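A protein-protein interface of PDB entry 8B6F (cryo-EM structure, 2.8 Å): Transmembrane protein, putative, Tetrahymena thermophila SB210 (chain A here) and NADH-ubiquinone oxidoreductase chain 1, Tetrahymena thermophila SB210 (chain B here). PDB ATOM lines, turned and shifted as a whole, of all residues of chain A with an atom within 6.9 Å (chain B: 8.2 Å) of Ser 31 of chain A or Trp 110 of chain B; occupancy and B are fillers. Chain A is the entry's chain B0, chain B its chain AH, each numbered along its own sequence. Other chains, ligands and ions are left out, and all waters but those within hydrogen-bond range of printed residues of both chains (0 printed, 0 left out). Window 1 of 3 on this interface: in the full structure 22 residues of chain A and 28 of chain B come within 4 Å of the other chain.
Printed residues of chain B within 4 Å of Gly 27 of chain A: Val 35.
Of the printed residues of chain A, Ile 32 of chain B touches Phe 30.
Met 109 of chain B touches none of the printed residues of chain A.
Trp 110 of chain B touches just these residues of chain A: Phe 30 (3.5 Å), Ser 31 (3.7 Å) and Ile 34 (3.6 Å).
Phe 254 of chain B touches none of the printed residues of chain A.
Printed residues of chain A that touch a printed residue of chain B: Tyr 23, Phe 26, Gly 27, Gly 29, Phe 30, Ser 31, Val 33, Ile 34 and Val 37.
Printed residues of chain B that touch a printed residue of chain A: Cys 28, Leu 31, Ile 32, Val 35, Trp 105, Trp 110, Val 114, Ile 116 and Phe 253.
Hydrophobic or aromatic side chains of chain B within 4 Å of the printed part of chain A: Leu 31, Ile 32, Val 35, Trp 105, Trp 110, Val 114, Ile 116 and Phe 253.
Among the printed residues, 16 pairs touch across the chains.
The backbone carbonyl oxygen (O) of Trp 105 of chain B lies within hydrogen-bond range of the side-chain hydroxyl (OG) of Ser 108 of chain B (2.5 Å).
OG of Ser 108 of chain B sits at hydrogen-bond distance from NE1 of Trp 110 of chain B (3.5 Å).
OG of Ser 31 of chain A lies within hydrogen-bond range of O of Gly 27 of chain A (3.0 Å).
Among the printed residues, merely in contact across the chains: Tyr 23 of chain A with Phe 253 of chain B, Phe 26 of chain A with Val 35 of chain B, Gly 27 of chain A with Val 35 of chain B, Gly 29 of chain A with Leu 31 of chain B, Phe 30 of chain A with Cys 28 of chain B, Phe 30 of chain A with Leu 31 of chain B, Phe 30 of chain A with Ile 32 of chain B, Phe 30 of chain A with Trp 105 of chain B, Phe 30 of chain A with Trp 110 of chain B, Ser 31 of chain A with Trp 110 of chain B, Val 33 of chain A with Cys 28 of chain B, Val 33 of chain A with Leu 31 of chain B, Ile 34 of chain A with Trp 105 of chain B, Ile 34 of chain A with Trp 110 of chain B, Ile 34 of chain A with Val 114 of chain B and Val 37 of chain A with Ile 116 of chain B.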
ATOM      1  N   TYR A  23      18.943   7.586 -15.774  1.00  0.00           N
ATOM      2  CA  TYR A  23      19.826   8.235 -14.812  1.00  0.00           C
ATOM      3  C   TYR A  23      20.916   9.024 -15.521  1.00  0.00           C
ATOM      4  O   TYR A  23      21.233  10.152 -15.125  1.00  0.00           O
ATOM      5  CB  TYR A  23      20.444   7.192 -13.881  1.00  0.00           C
ATOM      6  CG  TYR A  23      21.766   7.618 -13.283  1.00  0.00           C
ATOM      7  CD1 TYR A  23      22.964   7.369 -13.942  1.00  0.00           C
ATOM      8  CD2 TYR A  23      21.818   8.253 -12.052  1.00  0.00           C
ATOM      9  CE1 TYR A  23      24.171   7.756 -13.400  1.00  0.00           C
ATOM     10  CE2 TYR A  23      23.020   8.645 -11.502  1.00  0.00           C
ATOM     11  CZ  TYR A  23      24.192   8.392 -12.180  1.00  0.00           C
ATOM     12  OH  TYR A  23      25.392   8.776 -11.635  1.00  0.00           O
ATOM     13  N   PHE A  26      19.431  12.289 -16.949  1.00  0.00           N
ATOM     14  CA  PHE A  26      19.219  13.311 -15.929  1.00  0.00           C
ATOM     15  C   PHE A  26      20.543  13.844 -15.396  1.00  0.00           C
ATOM     16  O   PHE A  26      20.686  15.051 -15.172  1.00  0.00           O
ATOM     17  CB  PHE A  26      18.370  12.753 -14.786  1.00  0.00           C
ATOM     18  CG  PHE A  26      16.965  12.389 -15.185  1.00  0.00           C
ATOM     19  CD1 PHE A  26      16.345  13.000 -16.264  1.00  0.00           C
ATOM     20  CD2 PHE A  26      16.264  11.432 -14.472  1.00  0.00           C
ATOM     21  CE1 PHE A  26      15.057  12.663 -16.621  1.00  0.00           C
ATOM     22  CE2 PHE A  26      14.974  11.091 -14.827  1.00  0.00           C
ATOM     23  CZ  PHE A  26      14.371  11.707 -15.902  1.00  0.00           C
ATOM     24  N   GLY A  27      21.519  12.960 -15.184  1.00  0.00           N
ATOM     25  CA  GLY A  27      22.800  13.404 -14.662  1.00  0.00           C
ATOM     26  C   GLY A  27      23.553  14.288 -15.635  1.00  0.00           C
ATOM     27  O   GLY A  27      24.161  15.285 -15.237  1.00  0.00           O
ATOM     28  N   LEU A  28      23.538  13.932 -16.920  1.00  0.00           N
ATOM     29  CA  LEU A  28      24.150  14.793 -17.925  1.00  0.00           C
ATOM     30  C   LEU A  28      23.439  16.137 -18.000  1.00  0.00           C
ATOM     31  O   LEU A  28      24.085  17.182 -18.143  1.00  0.00           O
ATOM     32  CB  LEU A  28      24.144  14.098 -19.287  1.00  0.00           C
ATOM     33  CG  LEU A  28      25.191  12.996 -19.475  1.00  0.00           C
ATOM     34  CD1 LEU A  28      25.005  12.311 -20.814  1.00  0.00           C
ATOM     35  CD2 LEU A  28      26.602  13.554 -19.364  1.00  0.00           C
ATOM     36  N   GLY A  29      22.109  16.133 -17.915  1.00  0.00           N
ATOM     37  CA  GLY A  29      21.384  17.391 -17.887  1.00  0.00           C
ATOM     38  C   GLY A  29      21.807  18.264 -16.723  1.00  0.00           C
ATOM     39  O   GLY A  29      22.065  19.459 -16.885  1.00  0.00           O
ATOM     40  N   PHE A  30      21.885  17.677 -15.528  1.00  0.00           N
ATOM     41  CA  PHE A  30      22.263  18.443 -14.345  1.00  0.00           C
ATOM     42  C   PHE A  30      23.680  18.986 -14.477  1.00  0.00           C
ATOM     43  O   PHE A  30      23.938  20.161 -14.191  1.00  0.00           O
ATOM     44  CB  PHE A  30      22.129  17.568 -13.099  1.00  0.00           C
ATOM     45  CG  PHE A  30      22.487  18.271 -11.825  1.00  0.00           C
ATOM     46  CD1 PHE A  30      21.566  19.078 -11.183  1.00  0.00           C
ATOM     47  CD2 PHE A  30      23.739  18.108 -11.257  1.00  0.00           C
ATOM     48  CE1 PHE A  30      21.889  19.722 -10.005  1.00  0.00           C
ATOM     49  CE2 PHE A  30      24.068  18.748 -10.079  1.00  0.00           C
ATOM     50  CZ  PHE A  30      23.142  19.557  -9.452  1.00  0.00           C
ATOM     51  N   SER A  31      24.617  18.137 -14.897  1.00  0.00           N
ATOM     52  CA  SER A  31      26.005  18.569 -15.022  1.00  0.00           C
ATOM     53  C   SER A  31      26.155  19.653 -16.082  1.00  0.00           C
ATOM     54  O   SER A  31      26.887  20.628 -15.884  1.00  0.00           O
ATOM     55  CB  SER A  31      26.894  17.373 -15.354  1.00  0.00           C
ATOM     56  OG  SER A  31      26.836  16.398 -14.328  1.00  0.00           O
ATOM     57  N   THR A  32      25.480  19.492 -17.221  1.00  0.00           N
ATOM     58  CA  THR A  32      25.557  20.503 -18.271  1.00  0.00           C
ATOM     59  C   THR A  32      24.930  21.817 -17.826  1.00  0.00           C
ATOM     60  O   THR A  32      25.433  22.894 -18.165  1.00  0.00           O
ATOM     61  CB  THR A  32      24.889  19.987 -19.545  1.00  0.00           C
ATOM     62  OG1 THR A  32      25.606  18.846 -20.029  1.00  0.00           O
ATOM     63  CG2 THR A  32      24.865  21.061 -20.627  1.00  0.00           C
ATOM     64  N   VAL A  33      23.833  21.757 -17.072  1.00  0.00           N
ATOM     65  CA  VAL A  33      23.219  22.986 -16.579  1.00  0.00           C
ATOM     66  C   VAL A  33      24.179  23.715 -15.649  1.00  0.00           C
ATOM     67  O   VAL A  33      24.370  24.931 -15.756  1.00  0.00           O
ATOM     68  CB  VAL A  33      21.876  22.679 -15.894  1.00  0.00           C
ATOM     69  CG1 VAL A  33      21.414  23.845 -15.026  1.00  0.00           C
ATOM     70  CG2 VAL A  33      20.829  22.361 -16.939  1.00  0.00           C
ATOM     71  N   ILE A  34      24.813  22.984 -14.732  1.00  0.00           N
ATOM     72  CA  ILE A  34      25.777  23.618 -13.837  1.00  0.00           C
ATOM     73  C   ILE A  34      26.925  24.207 -14.642  1.00  0.00           C
ATOM     74  O   ILE A  34      27.355  25.340 -14.400  1.00  0.00           O
ATOM     75  CB  ILE A  34      26.276  22.614 -12.781  1.00  0.00           C
ATOM     76  CG1 ILE A  34      25.288  22.561 -11.613  1.00  0.00           C
ATOM     77  CG2 ILE A  34      27.685  22.982 -12.295  1.00  0.00           C
ATOM     78  CD1 ILE A  34      25.676  21.608 -10.505  1.00  0.00           C
ATOM     79  N   TYR A  35      27.441  23.447 -15.608  1.00  0.00           N
ATOM     80  CA  TYR A  35      28.567  23.918 -16.406  1.00  0.00           C
ATOM     81  C   TYR A  35      28.210  25.200 -17.147  1.00  0.00           C
ATOM     82  O   TYR A  35      28.988  26.158 -17.167  1.00  0.00           O
ATOM     83  CB  TYR A  35      28.996  22.823 -17.385  1.00  0.00           C
ATOM     84  CG  TYR A  35      30.144  23.201 -18.292  1.00  0.00           C
ATOM     85  CD1 TYR A  35      29.920  23.880 -19.485  1.00  0.00           C
ATOM     86  CD2 TYR A  35      31.448  22.866 -17.966  1.00  0.00           C
ATOM     87  CE1 TYR A  35      30.967  24.221 -20.319  1.00  0.00           C
ATOM     88  CE2 TYR A  35      32.501  23.202 -18.792  1.00  0.00           C
ATOM     89  CZ  TYR A  35      32.253  23.880 -19.966  1.00  0.00           C
ATOM     90  OH  TYR A  35      33.298  24.217 -20.794  1.00  0.00           O
ATOM     91  N   ASP A  36      27.030  25.233 -17.767  1.00  0.00           N
ATOM     92  CA  ASP A  36      26.625  26.416 -18.519  1.00  0.00           C
ATOM     93  C   ASP A  36      26.364  27.603 -17.601  1.00  0.00           C
ATOM     94  O   ASP A  36      26.720  28.738 -17.932  1.00  0.00           O
ATOM     95  CB  ASP A  36      25.385  26.102 -19.352  1.00  0.00           C
ATOM     96  CG  ASP A  36      25.621  24.985 -20.340  1.00  0.00           C
ATOM     97  OD1 ASP A  36      26.733  24.917 -20.900  1.00  0.00           O
ATOM     98  OD2 ASP A  36      24.698  24.179 -20.558  1.00  0.00           O
ATOM     99  N   VAL A  37      25.746  27.365 -16.443  1.00  0.00           N
ATOM    100  CA  VAL A  37      25.460  28.461 -15.522  1.00  0.00           C
ATOM    101  C   VAL A  37      26.753  29.107 -15.044  1.00  0.00           C
ATOM    102  O   VAL A  37      26.845  30.336 -14.936  1.00  0.00           O
ATOM    103  CB  VAL A  37      24.605  27.959 -14.343  1.00  0.00           C
ATOM    104  CG1 VAL A  37      24.496  29.020 -13.256  1.00  0.00           C
ATOM    105  CG2 VAL A  37      23.214  27.583 -14.823  1.00  0.00           C
ATOM    106  N   CYS B  28      18.248  23.558 -11.528  1.00  0.00           N
ATOM    107  CA  CYS B  28      19.216  22.616 -10.974  1.00  0.00           C
ATOM    108  C   CYS B  28      18.560  21.697  -9.951  1.00  0.00           C
ATOM    109  O   CYS B  28      18.800  20.485  -9.951  1.00  0.00           O
ATOM    110  CB  CYS B  28      20.381  23.372 -10.340  1.00  0.00           C
ATOM    111  SG  CYS B  28      21.441  24.233 -11.518  1.00  0.00           S
ATOM    112  N   LEU B  31      16.356  19.126 -11.690  1.00  0.00           N
ATOM    113  CA  LEU B  31      17.151  18.095 -12.351  1.00  0.00           C
ATOM    114  C   LEU B  31      17.728  17.104 -11.350  1.00  0.00           C
ATOM    115  O   LEU B  31      17.721  15.893 -11.595  1.00  0.00           O
ATOM    116  CB  LEU B  31      18.268  18.736 -13.172  1.00  0.00           C
ATOM    117  CG  LEU B  31      17.816  19.477 -14.431  1.00  0.00           C
ATOM    118  CD1 LEU B  31      18.985  20.182 -15.071  1.00  0.00           C
ATOM    119  CD2 LEU B  31      17.173  18.529 -15.430  1.00  0.00           C
ATOM    120  N   ILE B  32      18.230  17.591 -10.216  1.00  0.00           N
ATOM    121  CA  ILE B  32      18.772  16.672  -9.222  1.00  0.00           C
ATOM    122  C   ILE B  32      17.657  15.827  -8.622  1.00  0.00           C
ATOM    123  O   ILE B  32      17.868  14.654  -8.291  1.00  0.00           O
ATOM    124  CB  ILE B  32      19.572  17.433  -8.144  1.00  0.00           C
ATOM    125  CG1 ILE B  32      20.515  16.480  -7.406  1.00  0.00           C
ATOM    126  CG2 ILE B  32      18.658  18.132  -7.154  1.00  0.00           C
ATOM    127  CD1 ILE B  32      21.701  16.024  -8.229  1.00  0.00           C
ATOM    128  N   VAL B  35      17.197  13.089 -10.967  1.00  0.00           N
ATOM    129  CA  VAL B  35      18.286  12.127 -10.824  1.00  0.00           C
ATOM    130  C   VAL B  35      18.020  11.195  -9.649  1.00  0.00           C
ATOM    131  O   VAL B  35      18.220   9.980  -9.744  1.00  0.00           O
ATOM    132  CB  VAL B  35      19.630  12.863 -10.668  1.00  0.00           C
ATOM    133  CG1 VAL B  35      20.747  11.891 -10.311  1.00  0.00           C
ATOM    134  CG2 VAL B  35      19.979  13.609 -11.939  1.00  0.00           C
ATOM    135  N   TRP B 105      23.114  19.799  -2.721  1.00  0.00           N
ATOM    136  CA  TRP B 105      23.756  19.722  -4.027  1.00  0.00           C
ATOM    137  C   TRP B 105      24.757  20.840  -4.281  1.00  0.00           C
ATOM    138  O   TRP B 105      25.528  20.741  -5.240  1.00  0.00           O
ATOM    139  CB  TRP B 105      22.698  19.732  -5.134  1.00  0.00           C
ATOM    140  CG  TRP B 105      22.012  21.050  -5.311  1.00  0.00           C
ATOM    141  CD1 TRP B 105      20.866  21.460  -4.705  1.00  0.00           C
ATOM    142  CD2 TRP B 105      22.427  22.129  -6.157  1.00  0.00           C
ATOM    143  NE1 TRP B 105      20.539  22.729  -5.117  1.00  0.00           N
ATOM    144  CE2 TRP B 105      21.483  23.162  -6.009  1.00  0.00           C
ATOM    145  CE3 TRP B 105      23.507  22.320  -7.024  1.00  0.00           C
ATOM    146  CZ2 TRP B 105      21.585  24.371  -6.694  1.00  0.00           C
ATOM    147  CZ3 TRP B 105      23.607  23.521  -7.705  1.00  0.00           C
ATOM    148  CH2 TRP B 105      22.650  24.531  -7.536  1.00  0.00           C
ATOM    149  N   ILE B 106      24.770  21.898  -3.467  1.00  0.00           N
ATOM    150  CA  ILE B 106      25.726  22.977  -3.704  1.00  0.00           C
ATOM    151  C   ILE B 106      27.147  22.473  -3.506  1.00  0.00           C
ATOM    152  O   ILE B 106      28.076  22.895  -4.206  1.00  0.00           O
ATOM    153  CB  ILE B 106      25.421  24.187  -2.798  1.00  0.00           C
ATOM    154  CG1 ILE B 106      25.771  23.874  -1.336  1.00  0.00           C
ATOM    155  CG2 ILE B 106      23.963  24.593  -2.950  1.00  0.00           C
ATOM    156  CD1 ILE B 106      25.449  24.992  -0.356  1.00  0.00           C
ATOM    157  N   ASN B 107      27.341  21.566  -2.552  1.00  0.00           N
ATOM    158  CA  ASN B 107      28.664  21.024  -2.252  1.00  0.00           C
ATOM    159  C   ASN B 107      28.962  19.823  -3.149  1.00  0.00           C
ATOM    160  O   ASN B 107      29.139  18.694  -2.697  1.00  0.00           O
ATOM    161  CB  ASN B 107      28.749  20.653  -0.775  1.00  0.00           C
ATOM    162  CG  ASN B 107      30.144  20.253  -0.355  1.00  0.00           C
ATOM    163  OD1 ASN B 107      31.132  20.700  -0.936  1.00  0.00           O
ATOM    164  ND2 ASN B 107      30.235  19.407   0.662  1.00  0.00           N
ATOM    165  N   SER B 108      29.010  20.090  -4.452  1.00  0.00           N
ATOM    166  CA  SER B 108      29.291  19.063  -5.443  1.00  0.00           C
ATOM    167  C   SER B 108      30.133  19.654  -6.561  1.00  0.00           C
ATOM    168  O   SER B 108      29.898  20.787  -6.990  1.00  0.00           O
ATOM    169  CB  SER B 108      27.998  18.468  -6.015  1.00  0.00           C
ATOM    170  OG  SER B 108      27.207  19.469  -6.629  1.00  0.00           O
ATOM    171  N   MET B 109      31.109  18.883  -7.031  1.00  0.00           N
ATOM    172  CA  MET B 109      31.984  19.289  -8.121  1.00  0.00           C
ATOM    173  C   MET B 109      31.866  18.297  -9.267  1.00  0.00           C
ATOM    174  O   MET B 109      31.789  17.085  -9.047  1.00  0.00           O
ATOM    175  CB  MET B 109      33.441  19.388  -7.672  1.00  0.00           C
ATOM    176  CG  MET B 109      33.686  20.492  -6.658  1.00  0.00           C
ATOM    177  SD  MET B 109      35.381  21.104  -6.666  1.00  0.00           S
ATOM    178  CE  MET B 109      35.459  21.835  -8.300  1.00  0.00           C
ATOM    179  N   TRP B 110      31.853  18.822 -10.491  1.00  0.00           N
ATOM    180  CA  TRP B 110      31.688  18.016 -11.694  1.00  0.00           C
ATOM    181  C   TRP B 110      32.819  18.273 -12.682  1.00  0.00           C
ATOM    182  O   TRP B 110      32.628  18.174 -13.895  1.00  0.00           O
ATOM    183  CB  TRP B 110      30.333  18.297 -12.344  1.00  0.00           C
ATOM    184  CG  TRP B 110      29.190  18.145 -11.396  1.00  0.00           C
ATOM    185  CD1 TRP B 110      28.518  19.144 -10.756  1.00  0.00           C
ATOM    186  CD2 TRP B 110      28.587  16.919 -10.971  1.00  0.00           C
ATOM    187  NE1 TRP B 110      27.531  18.616  -9.961  1.00  0.00           N
ATOM    188  CE2 TRP B 110      27.554  17.251 -10.075  1.00  0.00           C
ATOM    189  CE3 TRP B 110      28.821  15.572 -11.263  1.00  0.00           C
ATOM    190  CZ2 TRP B 110      26.754  16.287  -9.468  1.00  0.00           C
ATOM    191  CZ3 TRP B 110      28.028  14.615 -10.661  1.00  0.00           C
ATOM    192  CH2 TRP B 110      27.006  14.976  -9.772  1.00  0.00           C
ATOM    193  N   GLY B 111      34.002  18.597 -12.172  1.00  0.00           N
ATOM    194  CA  GLY B 111      35.138  18.916 -13.002  1.00  0.00           C
ATOM    195  C   GLY B 111      36.204  19.628 -12.200  1.00  0.00           C
ATOM    196  O   GLY B 111      36.084  19.795 -10.983  1.00  0.00           O
ATOM    197  N   PRO B 112      37.272  20.071 -12.866  1.00  0.00           N
ATOM    198  CA  PRO B 112      38.344  20.756 -12.125  1.00  0.00           C
ATOM    199  C   PRO B 112      37.852  21.948 -11.323  1.00  0.00           C
ATOM    200  O   PRO B 112      38.294  22.146 -10.185  1.00  0.00           O
ATOM    201  CB  PRO B 112      39.319  21.172 -13.236  1.00  0.00           C
ATOM    202  CG  PRO B 112      39.063  20.216 -14.344  1.00  0.00           C
ATOM    203  CD  PRO B 112      37.600  19.907 -14.290  1.00  0.00           C
ATOM    204  N   SER B 113      36.949  22.753 -11.886  1.00  0.00           N
ATOM    205  CA  SER B 113      36.346  23.861 -11.156  1.00  0.00           C
ATOM    206  C   SER B 113      34.867  24.002 -11.486  1.00  0.00           C
ATOM    207  O   SER B 113      34.304  25.098 -11.386  1.00  0.00           O
ATOM    208  CB  SER B 113      37.081  25.167 -11.442  1.00  0.00           C
ATOM    209  OG  SER B 113      38.415  25.077 -10.977  1.00  0.00           O
ATOM    210  N   VAL B 114      34.223  22.908 -11.879  1.00  0.00           N
ATOM    211  CA  VAL B 114      32.820  22.954 -12.318  1.00  0.00           C
ATOM    212  C   VAL B 114      31.980  22.770 -11.060  1.00  0.00           C
ATOM    213  O   VAL B 114      31.547  21.673 -10.701  1.00  0.00           O
ATOM    214  CB  VAL B 114      32.518  21.906 -13.393  1.00  0.00           C
ATOM    215  CG1 VAL B 114      31.102  22.074 -13.916  1.00  0.00           C
ATOM    216  CG2 VAL B 114      33.528  21.999 -14.526  1.00  0.00           C
ATOM    217  N   SER B 115      31.746  23.882 -10.369  1.00  0.00           N
ATOM    218  CA  SER B 115      30.908  23.906  -9.182  1.00  0.00           C
ATOM    219  C   SER B 115      30.055  25.164  -9.218  1.00  0.00           C
ATOM    220  O   SER B 115      30.489  26.210  -9.704  1.00  0.00           O
ATOM    221  CB  SER B 115      31.749  23.876  -7.901  1.00  0.00           C
ATOM    222  OG  SER B 115      30.930  23.839  -6.747  1.00  0.00           O
ATOM    223  N   ILE B 116      28.837  25.057  -8.684  1.00  0.00           N
ATOM    224  CA  ILE B 116      27.927  26.198  -8.699  1.00  0.00           C
ATOM    225  C   ILE B 116      28.524  27.365  -7.924  1.00  0.00           C
ATOM    226  O   ILE B 116      28.368  28.529  -8.309  1.00  0.00           O
ATOM    227  CB  ILE B 116      26.548  25.787  -8.147  1.00  0.00           C
ATOM    228  CG1 ILE B 116      25.531  26.917  -8.328  1.00  0.00           C
ATOM    229  CG2 ILE B 116      26.641  25.390  -6.679  1.00  0.00           C
ATOM    230  CD1 ILE B 116      25.231  27.254  -9.774  1.00  0.00           C
ATOM    231  N   PHE B 183      37.510  19.190  -3.328  1.00  0.00           N
ATOM    232  CA  PHE B 183      37.497  17.914  -4.035  1.00  0.00           C
ATOM    233  C   PHE B 183      38.452  17.902  -5.223  1.00  0.00           C
ATOM    234  O   PHE B 183      38.962  16.839  -5.590  1.00  0.00           O
ATOM    235  CB  PHE B 183      36.079  17.594  -4.508  1.00  0.00           C
ATOM    236  CG  PHE B 183      35.093  17.382  -3.396  1.00  0.00           C
ATOM    237  CD1 PHE B 183      35.479  16.795  -2.202  1.00  0.00           C
ATOM    238  CD2 PHE B 183      33.770  17.757  -3.556  1.00  0.00           C
ATOM    239  CE1 PHE B 183      34.567  16.597  -1.187  1.00  0.00           C
ATOM    240  CE2 PHE B 183      32.853  17.561  -2.544  1.00  0.00           C
ATOM    241  CZ  PHE B 183      33.252  16.978  -1.358  1.00  0.00           C
ATOM    242  N   SER B 184      38.700  19.059  -5.838  1.00  0.00           N
ATOM    243  CA  SER B 184      39.517  19.088  -7.047  1.00  0.00           C
ATOM    244  C   SER B 184      40.939  18.617  -6.776  1.00  0.00           C
ATOM    245  O   SER B 184      41.533  17.906  -7.593  1.00  0.00           O
ATOM    246  CB  SER B 184      39.535  20.499  -7.629  1.00  0.00           C
ATOM    247  OG  SER B 184      38.229  20.937  -7.944  1.00  0.00           O
ATOM    248  N   PHE B 253      23.559   9.714  -2.949  1.00  0.00           N
ATOM    249  CA  PHE B 253      24.142  10.074  -4.236  1.00  0.00           C
ATOM    250  C   PHE B 253      25.375  10.949  -4.056  1.00  0.00           C
ATOM    251  O   PHE B 253      26.411  10.718  -4.687  1.00  0.00           O
ATOM    252  CB  PHE B 253      23.090  10.791  -5.084  1.00  0.00           C
ATOM    253  CG  PHE B 253      23.597  11.261  -6.417  1.00  0.00           C
ATOM    254  CD1 PHE B 253      23.571  10.424  -7.517  1.00  0.00           C
ATOM    255  CD2 PHE B 253      24.079  12.550  -6.573  1.00  0.00           C
ATOM    256  CE1 PHE B 253      24.026  10.858  -8.745  1.00  0.00           C
ATOM    257  CE2 PHE B 253      24.536  12.988  -7.798  1.00  0.00           C
ATOM    258  CZ  PHE B 253      24.512  12.141  -8.885  1.00  0.00           C
ATOM    259  N   PHE B 254      25.278  11.970  -3.204  1.00  0.00           N
ATOM    260  CA  PHE B 254      26.378  12.920  -3.097  1.00  0.00           C
ATOM    261  C   PHE B 254      27.563  12.345  -2.332  1.00  0.00           C
ATOM    262  O   PHE B 254      28.707  12.700  -2.628  1.00  0.00           O
ATOM    263  CB  PHE B 254      25.890  14.219  -2.460  1.00  0.00           C
ATOM    264  CG  PHE B 254      25.020  15.032  -3.370  1.00  0.00           C
ATOM    265  CD1 PHE B 254      25.551  15.612  -4.511  1.00  0.00           C
ATOM    266  CD2 PHE B 254      23.676  15.203  -3.099  1.00  0.00           C
ATOM    267  CE1 PHE B 254      24.757  16.352  -5.358  1.00  0.00           C
ATOM    268  CE2 PHE B 254      22.875  15.942  -3.944  1.00  0.00           C
ATOM    269  CZ  PHE B 254      23.417  16.518  -5.075  1.00  0.00           C
ATOM    270  N   MET B 257      29.388  10.292  -4.787  1.00  0.00           N
ATOM    271  CA  MET B 257      30.244  11.190  -5.553  1.00  0.00           C
ATOM    272  C   MET B 257      31.498  11.551  -4.769  1.00  0.00           C
ATOM    273  O   MET B 257      32.603  11.572  -5.322  1.00  0.00           O
ATOM    274  CB  MET B 257      29.466  12.450  -5.930  1.00  0.00           C
ATOM    275  CG  MET B 257      30.265  13.484  -6.720  1.00  0.00           C
ATOM    276  SD  MET B 257      29.711  15.169  -6.409  1.00  0.00           S
ATOM    277  CE  MET B 257      30.202  15.371  -4.698  1.00  0.00           C
ATOM    278  N   ILE B 261      35.356  10.733  -5.936  1.00  0.00           N
ATOM    279  CA  ILE B 261      36.340  11.782  -6.184  1.00  0.00           C
ATOM    280  C   ILE B 261      37.566  11.608  -5.295  1.00  0.00           C
ATOM    281  O   ILE B 261      38.705  11.752  -5.754  1.00  0.00           O
ATOM    282  CB  ILE B 261      35.702  13.170  -5.999  1.00  0.00           C
ATOM    283  CG1 ILE B 261      34.633  13.417  -7.066  1.00  0.00           C
ATOM    284  CG2 ILE B 261      36.766  14.243  -6.096  1.00  0.00           C
ATOM    285  CD1 ILE B 261      33.790  14.657  -6.824  1.00  0.00           C
ATOM    286  N   TRP B 267      37.088  12.023 -11.867  1.00  0.00           N
ATOM    287  CA  TRP B 267      36.844  12.087 -13.303  1.00  0.00           C
ATOM    288  C   TRP B 267      38.066  11.676 -14.118  1.00  0.00           C
ATOM    289  O   TRP B 267      38.226  12.117 -15.261  1.00  0.00           O
ATOM    290  CB  TRP B 267      36.387  13.491 -13.695  1.00  0.00           C
ATOM    291  CG  TRP B 267      37.237  14.593 -13.134  1.00  0.00           C
ATOM    292  CD1 TRP B 267      38.394  15.082 -13.661  1.00  0.00           C
ATOM    293  CD2 TRP B 267      36.992  15.341 -11.938  1.00  0.00           C
ATOM    294  NE1 TRP B 267      38.886  16.089 -12.867  1.00  0.00           N
ATOM    295  CE2 TRP B 267      38.044  16.266 -11.802  1.00  0.00           C
ATOM    296  CE3 TRP B 267      35.985  15.316 -10.968  1.00  0.00           C
ATOM    297  CZ2 TRP B 267      38.119  17.161 -10.736  1.00  0.00           C
ATOM    298  CZ3 TRP B 267      36.060  16.204  -9.910  1.00  0.00           C
ATOM    299  CH2 TRP B 267      37.121  17.114  -9.802  1.00  0.00           C
